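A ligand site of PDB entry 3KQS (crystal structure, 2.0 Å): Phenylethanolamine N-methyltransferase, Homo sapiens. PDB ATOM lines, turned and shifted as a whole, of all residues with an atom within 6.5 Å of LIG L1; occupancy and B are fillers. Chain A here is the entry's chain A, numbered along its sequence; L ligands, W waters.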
ATOM      1  N   TYR A  35       5.939 -15.170   2.853  1.00  0.00           N
ATOM      2  CA  TYR A  35       4.512 -15.003   3.135  1.00  0.00           C
ATOM      3  C   TYR A  35       3.677 -16.147   2.530  1.00  0.00           C
ATOM      4  O   TYR A  35       2.803 -16.706   3.196  1.00  0.00           O
ATOM      5  CB  TYR A  35       4.012 -13.664   2.611  1.00  0.00           C
ATOM      6  CG  TYR A  35       2.518 -13.446   2.793  1.00  0.00           C
ATOM      7  CD1 TYR A  35       2.008 -13.060   4.028  1.00  0.00           C
ATOM      8  CD2 TYR A  35       1.633 -13.631   1.733  1.00  0.00           C
ATOM      9  CE1 TYR A  35       0.653 -12.864   4.202  1.00  0.00           C
ATOM     10  CE2 TYR A  35       0.277 -13.434   1.908  1.00  0.00           C
ATOM     11  CZ  TYR A  35      -0.213 -13.060   3.138  1.00  0.00           C
ATOM     12  OH  TYR A  35      -1.558 -12.860   3.326  1.00  0.00           O
ATOM     13  N   ASN A  39       1.529 -19.269   4.684  1.00  0.00           N
ATOM     14  CA  ASN A  39       0.068 -19.219   4.728  1.00  0.00           C
ATOM     15  C   ASN A  39      -0.667 -20.080   3.701  1.00  0.00           C
ATOM     16  O   ASN A  39      -1.848 -20.395   3.897  1.00  0.00           O
ATOM     17  CB  ASN A  39      -0.416 -17.769   4.621  1.00  0.00           C
ATOM     18  CG  ASN A  39       0.059 -16.921   5.780  1.00  0.00           C
ATOM     19  OD1 ASN A  39      -0.448 -17.038   6.886  1.00  0.00           O
ATOM     20  ND2 ASN A  39       1.064 -16.089   5.532  1.00  0.00           N
ATOM     21  N   TYR A  40       0.017 -20.448   2.630  1.00  0.00           N
ATOM     22  CA  TYR A  40      -0.631 -21.105   1.490  1.00  0.00           C
ATOM     23  C   TYR A  40       0.093 -22.351   1.021  1.00  0.00           C
ATOM     24  O   TYR A  40      -0.202 -22.900  -0.047  1.00  0.00           O
ATOM     25  CB  TYR A  40      -0.847 -20.094   0.349  1.00  0.00           C
ATOM     26  CG  TYR A  40      -1.636 -18.893   0.848  1.00  0.00           C
ATOM     27  CD1 TYR A  40      -1.011 -17.700   1.174  1.00  0.00           C
ATOM     28  CD2 TYR A  40      -3.007 -18.988   1.055  1.00  0.00           C
ATOM     29  CE1 TYR A  40      -1.739 -16.607   1.650  1.00  0.00           C
ATOM     30  CE2 TYR A  40      -3.746 -17.908   1.534  1.00  0.00           C
ATOM     31  CZ  TYR A  40      -3.103 -16.725   1.833  1.00  0.00           C
ATOM     32  OH  TYR A  40      -3.833 -15.658   2.317  1.00  0.00           O
ATOM     33  N   ARG A  44      -1.424 -25.117   6.366  1.00  0.00           N
ATOM     34  CA  ARG A  44      -2.532 -24.207   6.041  1.00  0.00           C
ATOM     35  C   ARG A  44      -2.967 -24.345   4.589  1.00  0.00           C
ATOM     36  O   ARG A  44      -4.129 -24.154   4.265  1.00  0.00           O
ATOM     37  CB  ARG A  44      -2.166 -22.752   6.355  1.00  0.00           C
ATOM     38  CG  ARG A  44      -2.205 -22.429   7.846  1.00  0.00           C
ATOM     39  CD  ARG A  44      -1.625 -21.057   8.168  1.00  0.00           C
ATOM     40  NE  ARG A  44      -1.664 -20.822   9.611  1.00  0.00           N
ATOM     41  CZ  ARG A  44      -1.509 -19.642  10.188  1.00  0.00           C
ATOM     42  NH1 ARG A  44      -1.321 -18.558   9.445  1.00  0.00           N
ATOM     43  NH2 ARG A  44      -1.560 -19.536  11.514  1.00  0.00           N
ATOM     44  N   VAL A  53      -8.680 -24.392   7.024  1.00  0.00           N
ATOM     45  CA  VAL A  53      -8.988 -22.978   6.788  1.00  0.00           C
ATOM     46  C   VAL A  53      -9.099 -22.636   5.305  1.00  0.00           C
ATOM     47  O   VAL A  53      -9.902 -21.788   4.911  1.00  0.00           O
ATOM     48  CB  VAL A  53      -7.960 -22.049   7.475  1.00  0.00           C
ATOM     49  CG1 VAL A  53      -6.555 -22.297   6.931  1.00  0.00           C
ATOM     50  CG2 VAL A  53      -8.355 -20.603   7.300  1.00  0.00           C
ATOM     51  N   GLY A  54      -8.307 -23.293   4.467  1.00  0.00           N
ATOM     52  CA  GLY A  54      -8.378 -23.074   3.031  1.00  0.00           C
ATOM     53  C   GLY A  54      -9.723 -23.426   2.435  1.00  0.00           C
ATOM     54  O   GLY A  54     -10.362 -22.607   1.756  1.00  0.00           O
ATOM     55  N   LYS A  57     -12.464 -20.927   3.547  1.00  0.00           N
ATOM     56  CA  LYS A  57     -12.442 -19.666   2.804  1.00  0.00           C
ATOM     57  C   LYS A  57     -13.036 -19.792   1.399  1.00  0.00           C
ATOM     58  O   LYS A  57     -13.830 -18.952   0.978  1.00  0.00           O
ATOM     59  CB  LYS A  57     -11.008 -19.114   2.714  1.00  0.00           C
ATOM     60  CG  LYS A  57     -10.491 -18.488   4.015  1.00  0.00           C
ATOM     61  CD  LYS A  57      -9.146 -17.796   3.794  1.00  0.00           C
ATOM     62  CE  LYS A  57      -8.079 -18.820   3.403  1.00  0.00           C
ATOM     63  NZ  LYS A  57      -6.769 -18.175   3.189  1.00  0.00           N
ATOM     64  N   TYR A  85      -6.158 -16.806  -4.835  1.00  0.00           N
ATOM     65  CA  TYR A  85      -7.228 -17.712  -4.379  1.00  0.00           C
ATOM     66  C   TYR A  85      -8.531 -16.944  -4.126  1.00  0.00           C
ATOM     67  O   TYR A  85      -9.617 -17.499  -4.300  1.00  0.00           O
ATOM     68  CB  TYR A  85      -6.835 -18.462  -3.099  1.00  0.00           C
ATOM     69  CG  TYR A  85      -6.867 -17.567  -1.874  1.00  0.00           C
ATOM     70  CD1 TYR A  85      -8.002 -17.465  -1.092  1.00  0.00           C
ATOM     71  CD2 TYR A  85      -5.767 -16.777  -1.547  1.00  0.00           C
ATOM     72  CE1 TYR A  85      -8.051 -16.621   0.001  1.00  0.00           C
ATOM     73  CE2 TYR A  85      -5.815 -15.920  -0.458  1.00  0.00           C
ATOM     74  CZ  TYR A  85      -6.952 -15.849   0.318  1.00  0.00           C
ATOM     75  OH  TYR A  85      -7.011 -14.999   1.402  1.00  0.00           O
ATOM     76  N   TYR A 126      -5.611 -24.834  -5.136  1.00  0.00           N
ATOM     77  CA  TYR A 126      -6.722 -23.951  -4.813  1.00  0.00           C
ATOM     78  C   TYR A 126      -7.698 -23.903  -5.987  1.00  0.00           C
ATOM     79  O   TYR A 126      -8.916 -23.958  -5.798  1.00  0.00           O
ATOM     80  CB  TYR A 126      -6.218 -22.537  -4.471  1.00  0.00           C
ATOM     81  CG  TYR A 126      -5.626 -22.429  -3.076  1.00  0.00           C
ATOM     82  CD1 TYR A 126      -4.313 -22.829  -2.816  1.00  0.00           C
ATOM     83  CD2 TYR A 126      -6.381 -21.956  -2.018  1.00  0.00           C
ATOM     84  CE1 TYR A 126      -3.773 -22.734  -1.533  1.00  0.00           C
ATOM     85  CE2 TYR A 126      -5.842 -21.861  -0.735  1.00  0.00           C
ATOM     86  CZ  TYR A 126      -4.549 -22.253  -0.506  1.00  0.00           C
ATOM     87  OH  TYR A 126      -4.020 -22.157   0.777  1.00  0.00           O
ATOM     88  N   ALA A 181      -8.893  -9.451   1.235  1.00  0.00           N
ATOM     89  CA  ALA A 181      -8.592 -10.503   2.207  1.00  0.00           C
ATOM     90  C   ALA A 181      -7.300 -10.216   2.972  1.00  0.00           C
ATOM     91  O   ALA A 181      -6.249 -10.044   2.373  1.00  0.00           O
ATOM     92  CB  ALA A 181      -8.525 -11.878   1.530  1.00  0.00           C
ATOM     93  N   PHE A 182      -7.418 -10.176   4.304  1.00  0.00           N
ATOM     94  CA  PHE A 182      -6.259 -10.054   5.201  1.00  0.00           C
ATOM     95  C   PHE A 182      -5.462  -8.757   5.020  1.00  0.00           C
ATOM     96  O   PHE A 182      -4.269  -8.712   5.328  1.00  0.00           O
ATOM     97  CB  PHE A 182      -5.336 -11.268   5.055  1.00  0.00           C
ATOM     98  CG  PHE A 182      -5.982 -12.587   5.412  1.00  0.00           C
ATOM     99  CD1 PHE A 182      -6.242 -13.528   4.425  1.00  0.00           C
ATOM    100  CD2 PHE A 182      -6.321 -12.872   6.728  1.00  0.00           C
ATOM    101  CE1 PHE A 182      -6.819 -14.748   4.760  1.00  0.00           C
ATOM    102  CE2 PHE A 182      -6.908 -14.091   7.063  1.00  0.00           C
ATOM    103  CZ  PHE A 182      -7.157 -15.029   6.067  1.00  0.00           C
ATOM    104  N   GLU A 185      -6.966  -5.054   8.499  1.00  0.00           N
ATOM    105  CA  GLU A 185      -6.471  -5.236   9.855  1.00  0.00           C
ATOM    106  C   GLU A 185      -4.942  -5.322   9.885  1.00  0.00           C
ATOM    107  O   GLU A 185      -4.305  -4.986  10.882  1.00  0.00           O
ATOM    108  CB  GLU A 185      -7.113  -6.452  10.544  1.00  0.00           C
ATOM    109  CG  GLU A 185      -6.630  -7.814  10.038  1.00  0.00           C
ATOM    110  CD  GLU A 185      -7.333  -8.276   8.763  1.00  0.00           C
ATOM    111  OE1 GLU A 185      -8.156  -7.509   8.209  1.00  0.00           O
ATOM    112  OE2 GLU A 185      -7.060  -9.411   8.317  1.00  0.00           O
ATOM    113  N   ALA A 216      -8.254 -11.602   9.556  1.00  0.00           N
ATOM    114  CA  ALA A 216      -7.829 -12.311  10.757  1.00  0.00           C
ATOM    115  C   ALA A 216      -8.556 -11.770  11.979  1.00  0.00           C
ATOM    116  O   ALA A 216      -8.716 -10.557  12.117  1.00  0.00           O
ATOM    117  CB  ALA A 216      -6.318 -12.181  10.939  1.00  0.00           C
ATOM    118  N   GLU A 219      -5.791 -11.029  15.961  1.00  0.00           N
ATOM    119  CA  GLU A 219      -4.375 -11.202  15.630  1.00  0.00           C
ATOM    120  C   GLU A 219      -3.622  -9.913  15.968  1.00  0.00           C
ATOM    121  O   GLU A 219      -4.187  -8.816  15.891  1.00  0.00           O
ATOM    122  CB  GLU A 219      -4.224 -11.512  14.138  1.00  0.00           C
ATOM    123  CG  GLU A 219      -2.782 -11.714  13.688  1.00  0.00           C
ATOM    124  CD  GLU A 219      -2.654 -11.950  12.191  1.00  0.00           C
ATOM    125  OE1 GLU A 219      -1.984 -12.916  11.784  1.00  0.00           O
ATOM    126  OE2 GLU A 219      -3.247 -11.163  11.416  1.00  0.00           O
ATOM    127  N   TYR A 222       2.204 -10.898  12.476  1.00  0.00           N
ATOM    128  CA  TYR A 222       2.573 -12.014  11.609  1.00  0.00           C
ATOM    129  C   TYR A 222       3.942 -11.761  10.975  1.00  0.00           C
ATOM    130  O   TYR A 222       4.416 -10.625  10.933  1.00  0.00           O
ATOM    131  CB  TYR A 222       1.498 -12.303  10.543  1.00  0.00           C
ATOM    132  CG  TYR A 222       1.401 -11.299   9.414  1.00  0.00           C
ATOM    133  CD1 TYR A 222       1.907 -11.611   8.151  1.00  0.00           C
ATOM    134  CD2 TYR A 222       0.781 -10.072   9.590  1.00  0.00           C
ATOM    135  CE1 TYR A 222       1.813 -10.709   7.103  1.00  0.00           C
ATOM    136  CE2 TYR A 222       0.677  -9.164   8.533  1.00  0.00           C
ATOM    137  CZ  TYR A 222       1.203  -9.484   7.301  1.00  0.00           C
ATOM    138  OH  TYR A 222       1.096  -8.603   6.252  1.00  0.00           O
ATOM    139  N   MET A 258      -9.525 -21.040  14.550  1.00  0.00           N
ATOM    140  CA  MET A 258      -8.283 -21.673  14.107  1.00  0.00           C
ATOM    141  C   MET A 258      -7.934 -22.844  15.015  1.00  0.00           C
ATOM    142  O   MET A 258      -7.690 -22.669  16.207  1.00  0.00           O
ATOM    143  CB  MET A 258      -7.128 -20.662  14.066  1.00  0.00           C
ATOM    144  CG  MET A 258      -6.076 -20.960  13.013  1.00  0.00           C
ATOM    145  SD  MET A 258      -6.635 -20.552  11.344  1.00  0.00           S
ATOM    146  CE  MET A 258      -7.090 -18.839  11.566  1.00  0.00           C
ATOM    147  N   LEU A 262      -3.206 -25.683  13.111  1.00  0.00           N
ATOM    148  CA  LEU A 262      -2.914 -24.630  12.137  1.00  0.00           C
ATOM    149  C   LEU A 262      -2.349 -23.361  12.790  1.00  0.00           C
ATOM    150  O   LEU A 262      -2.166 -22.338  12.116  1.00  0.00           O
ATOM    151  CB  LEU A 262      -4.151 -24.289  11.288  1.00  0.00           C
ATOM    152  CG  LEU A 262      -4.692 -25.356  10.348  1.00  0.00           C
ATOM    153  CD1 LEU A 262      -5.919 -24.814   9.632  1.00  0.00           C
ATOM    154  CD2 LEU A 262      -3.641 -25.782   9.338  1.00  0.00           C
ATOM    155  N   ASP A 267       2.363 -16.485  13.121  1.00  0.00           N
ATOM    156  CA  ASP A 267       1.482 -15.413  13.579  1.00  0.00           C
ATOM    157  C   ASP A 267       0.767 -15.856  14.852  1.00  0.00           C
ATOM    158  O   ASP A 267       1.017 -16.951  15.353  1.00  0.00           O
ATOM    159  CB  ASP A 267       0.469 -15.002  12.502  1.00  0.00           C
ATOM    160  CG  ASP A 267      -0.453 -16.145  12.077  1.00  0.00           C
ATOM    161  OD1 ASP A 267      -0.752 -17.025  12.907  1.00  0.00           O
ATOM    162  OD2 ASP A 267      -0.883 -16.160  10.899  1.00  0.00           O
ATOM    163  N   VAL A 269      -2.809 -15.566  15.045  1.00  0.00           N
ATOM    164  CA  VAL A 269      -4.214 -15.498  14.633  1.00  0.00           C
ATOM    165  C   VAL A 269      -5.095 -16.475  15.411  1.00  0.00           C
ATOM    166  O   VAL A 269      -4.714 -17.634  15.630  1.00  0.00           O
ATOM    167  CB  VAL A 269      -4.352 -15.777  13.114  1.00  0.00           C
ATOM    168  CG1 VAL A 269      -3.892 -17.194  12.794  1.00  0.00           C
ATOM    169  CG2 VAL A 269      -5.784 -15.551  12.651  1.00  0.00           C
ATOM    170  N   GLY A 271      -8.715 -16.638  14.690  1.00  0.00           N
ATOM    171  CA  GLY A 271      -9.760 -17.062  13.779  1.00  0.00           C
ATOM    172  C   GLY A 271      -9.746 -16.259  12.497  1.00  0.00           C
ATOM    173  O   GLY A 271      -8.978 -15.294  12.360  1.00  0.00           O
ATOM    174  N   VAL A 272     -10.588 -16.651  11.553  1.00  0.00           N
ATOM    175  CA  VAL A 272     -10.751 -15.919  10.306  1.00  0.00           C
ATOM    176  C   VAL A 272     -12.216 -15.545  10.140  1.00  0.00           C
ATOM    177  O   VAL A 272     -13.091 -16.375  10.383  1.00  0.00           O
ATOM    178  CB  VAL A 272     -10.293 -16.768   9.087  1.00  0.00           C
ATOM    179  CG1 VAL A 272     -10.535 -16.021   7.788  1.00  0.00           C
ATOM    180  CG2 VAL A 272      -8.829 -17.144   9.217  1.00  0.00           C
HETATM  181  N1  LIG L   1      -3.503 -15.679   5.186  1.00  0.00           N
HETATM  182  C1  LIG L   1      -4.007 -16.834   5.970  1.00  0.00           C
HETATM  183  C2  LIG L   1      -4.511 -18.120   5.562  1.00  0.00           C
HETATM  184  C3  LIG L   1      -4.954 -19.074   6.551  1.00  0.00           C
HETATM  185  C4  LIG L   1      -4.874 -18.740   7.961  1.00  0.00           C
HETATM  186  C5  LIG L   1      -4.370 -17.455   8.369  1.00  0.00           C
HETATM  187  C6  LIG L   1      -3.937 -16.505   7.389  1.00  0.00           C
HETATM  188  N2  LIG L   1      -3.357 -15.102   7.510  1.00  0.00           N
HETATM  189  C7  LIG L   1      -3.101 -14.600   6.150  1.00  0.00           C
HETATM  190  N3  LIG L   1      -2.546 -13.297   5.816  1.00  0.00           N
HETATM  191  N1  LG2 L   2      -4.814 -10.455  -0.033  1.00  0.00           N
HETATM  192  C1  LG2 L   2      -3.653 -11.317   0.218  1.00  0.00           C
HETATM  193  C2  LG2 L   2      -2.527 -10.528   0.934  1.00  0.00           C
HETATM  194  C3  LG2 L   2      -2.862 -10.245   2.404  1.00  0.00           C
HETATM  195  S1  LG2 L   2      -1.367  -9.616   3.262  1.00  0.00           S
HETATM  196  C4  LG2 L   2      -4.104 -12.551   1.029  1.00  0.00           C
HETATM  197  O1  LG2 L   2      -5.233 -12.917   0.958  1.00  0.00           O
HETATM  198  O2  LG2 L   2      -3.116 -13.456   1.410  1.00  0.00           O
HETATM  199  C5  LG2 L   2      -1.554  -7.841   3.573  1.00  0.00           C
HETATM  200  C6  LG2 L   2      -1.281  -7.048   2.283  1.00  0.00           C
HETATM  201  O3  LG2 L   2      -1.551  -5.631   2.508  1.00  0.00           O
HETATM  202  C7  LG2 L   2       0.170  -7.146   1.789  1.00  0.00           C
HETATM  203  O4  LG2 L   2       0.170  -7.597   0.454  1.00  0.00           O
HETATM  204  C8  LG2 L   2       0.661  -5.715   1.877  1.00  0.00           C
HETATM  205  O5  LG2 L   2       1.608  -5.418   0.886  1.00  0.00           O
HETATM  206  C9  LG2 L   2      -0.627  -4.932   1.646  1.00  0.00           C
HETATM  207  N2  LG2 L   2      -0.479  -3.592   2.163  1.00  0.00           N
HETATM  208  C10 LG2 L   2       0.556  -3.074   3.115  1.00  0.00           C
HETATM  209  N3  LG2 L   2       0.285  -1.657   3.340  1.00  0.00           N
HETATM  210  C11 LG2 L   2      -0.909  -1.295   2.549  1.00  0.00           C
HETATM  211  C12 LG2 L   2      -1.659  -0.011   2.374  1.00  0.00           C
HETATM  212  N4  LG2 L   2      -1.240   1.184   3.084  1.00  0.00           N
HETATM  213  N5  LG2 L   2      -2.833   0.024   1.506  1.00  0.00           N
HETATM  214  C13 LG2 L   2      -3.296  -1.202   0.778  1.00  0.00           C
HETATM  215  N6  LG2 L   2      -2.555  -2.481   0.944  1.00  0.00           N
HETATM  216  C14 LG2 L   2      -1.370  -2.513   1.825  1.00  0.00           C
HETATM  217  O   HOH W   1      -1.215 -12.746   8.328  1.00  0.00           O
HETATM  218  O   HOH W   2      -2.163 -10.639   6.749  1.00  0.00           O
HETATM  219  O   HOH W   3      -3.152 -14.791  10.055  1.00  0.00           O
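Water W3 lies within hydrogen-bond range of N2 of LIG L1, OD2 of Asp 267 and OE1 of Glu 219.
Water W2 lies within hydrogen-bond range of N3 of LIG L1, O of Phe 182 and S1 of LG2 L2.
Residues that only touch LIG L1: Asn 39 (3.5 Å), Arg 44 (3.4 Å), Val 53 (3.6 Å), Lys 57 (3.3 Å) and Phe 182 (3.5 Å).
Seven residues have an atom within 4 Å of LIG L1: Tyr 35, Asn 39, Tyr 40, Arg 44, Val 53, Lys 57 and Phe 182.
The side-chain hydroxyl (OH) of Tyr 85 lies within hydrogen-bond range of an oxygen (O1) of LG2 L2, 2.8 Å away.
The side-chain hydroxyl (OH) of Tyr 35 lies within hydrogen-bond range of an oxygen (O2) of LG2 L2.
The backbone carbonyl oxygen (O) of Ala 181 sits at hydrogen-bond distance from a nitrogen (N1) of LG2 L2, 2.8 Å away.
The side-chain hydroxyl (OH) of Tyr 35 sits at hydrogen-bond distance from a nitrogen (N3) of LIG L1 (2.7 Å).
An oxygen (O2) of LG2 L2 is in hydrogen-bond range of the side-chain hydroxyl of Tyr 40 (2.5 Å).
The side-chain hydroxyl of Tyr 40 lies within hydrogen-bond range of a nitrogen (N1) of LIG L1, at 2.9 Å.
The backbone carbonyl oxygen (O) of Tyr 35 is in hydrogen-bond range of the side-chain amide nitrogen (ND2) of Asn 39 (3.0 Å).
The backbone carbonyl oxygen of Leu 262 sits at hydrogen-bond distance from the guanidinium group of Arg 44, 2.9 Å away.
OD2 of Asp 267 lies within salt-bridge range of NH1 of Arg 44 (2.8 Å).
NH1 of Arg 44 is in hydrogen-bond range of OD1 of Asn 39, at 3.1 Å.
OH of Tyr 85 sits at hydrogen-bond distance from OH of Tyr 40, 3.4 Å away.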
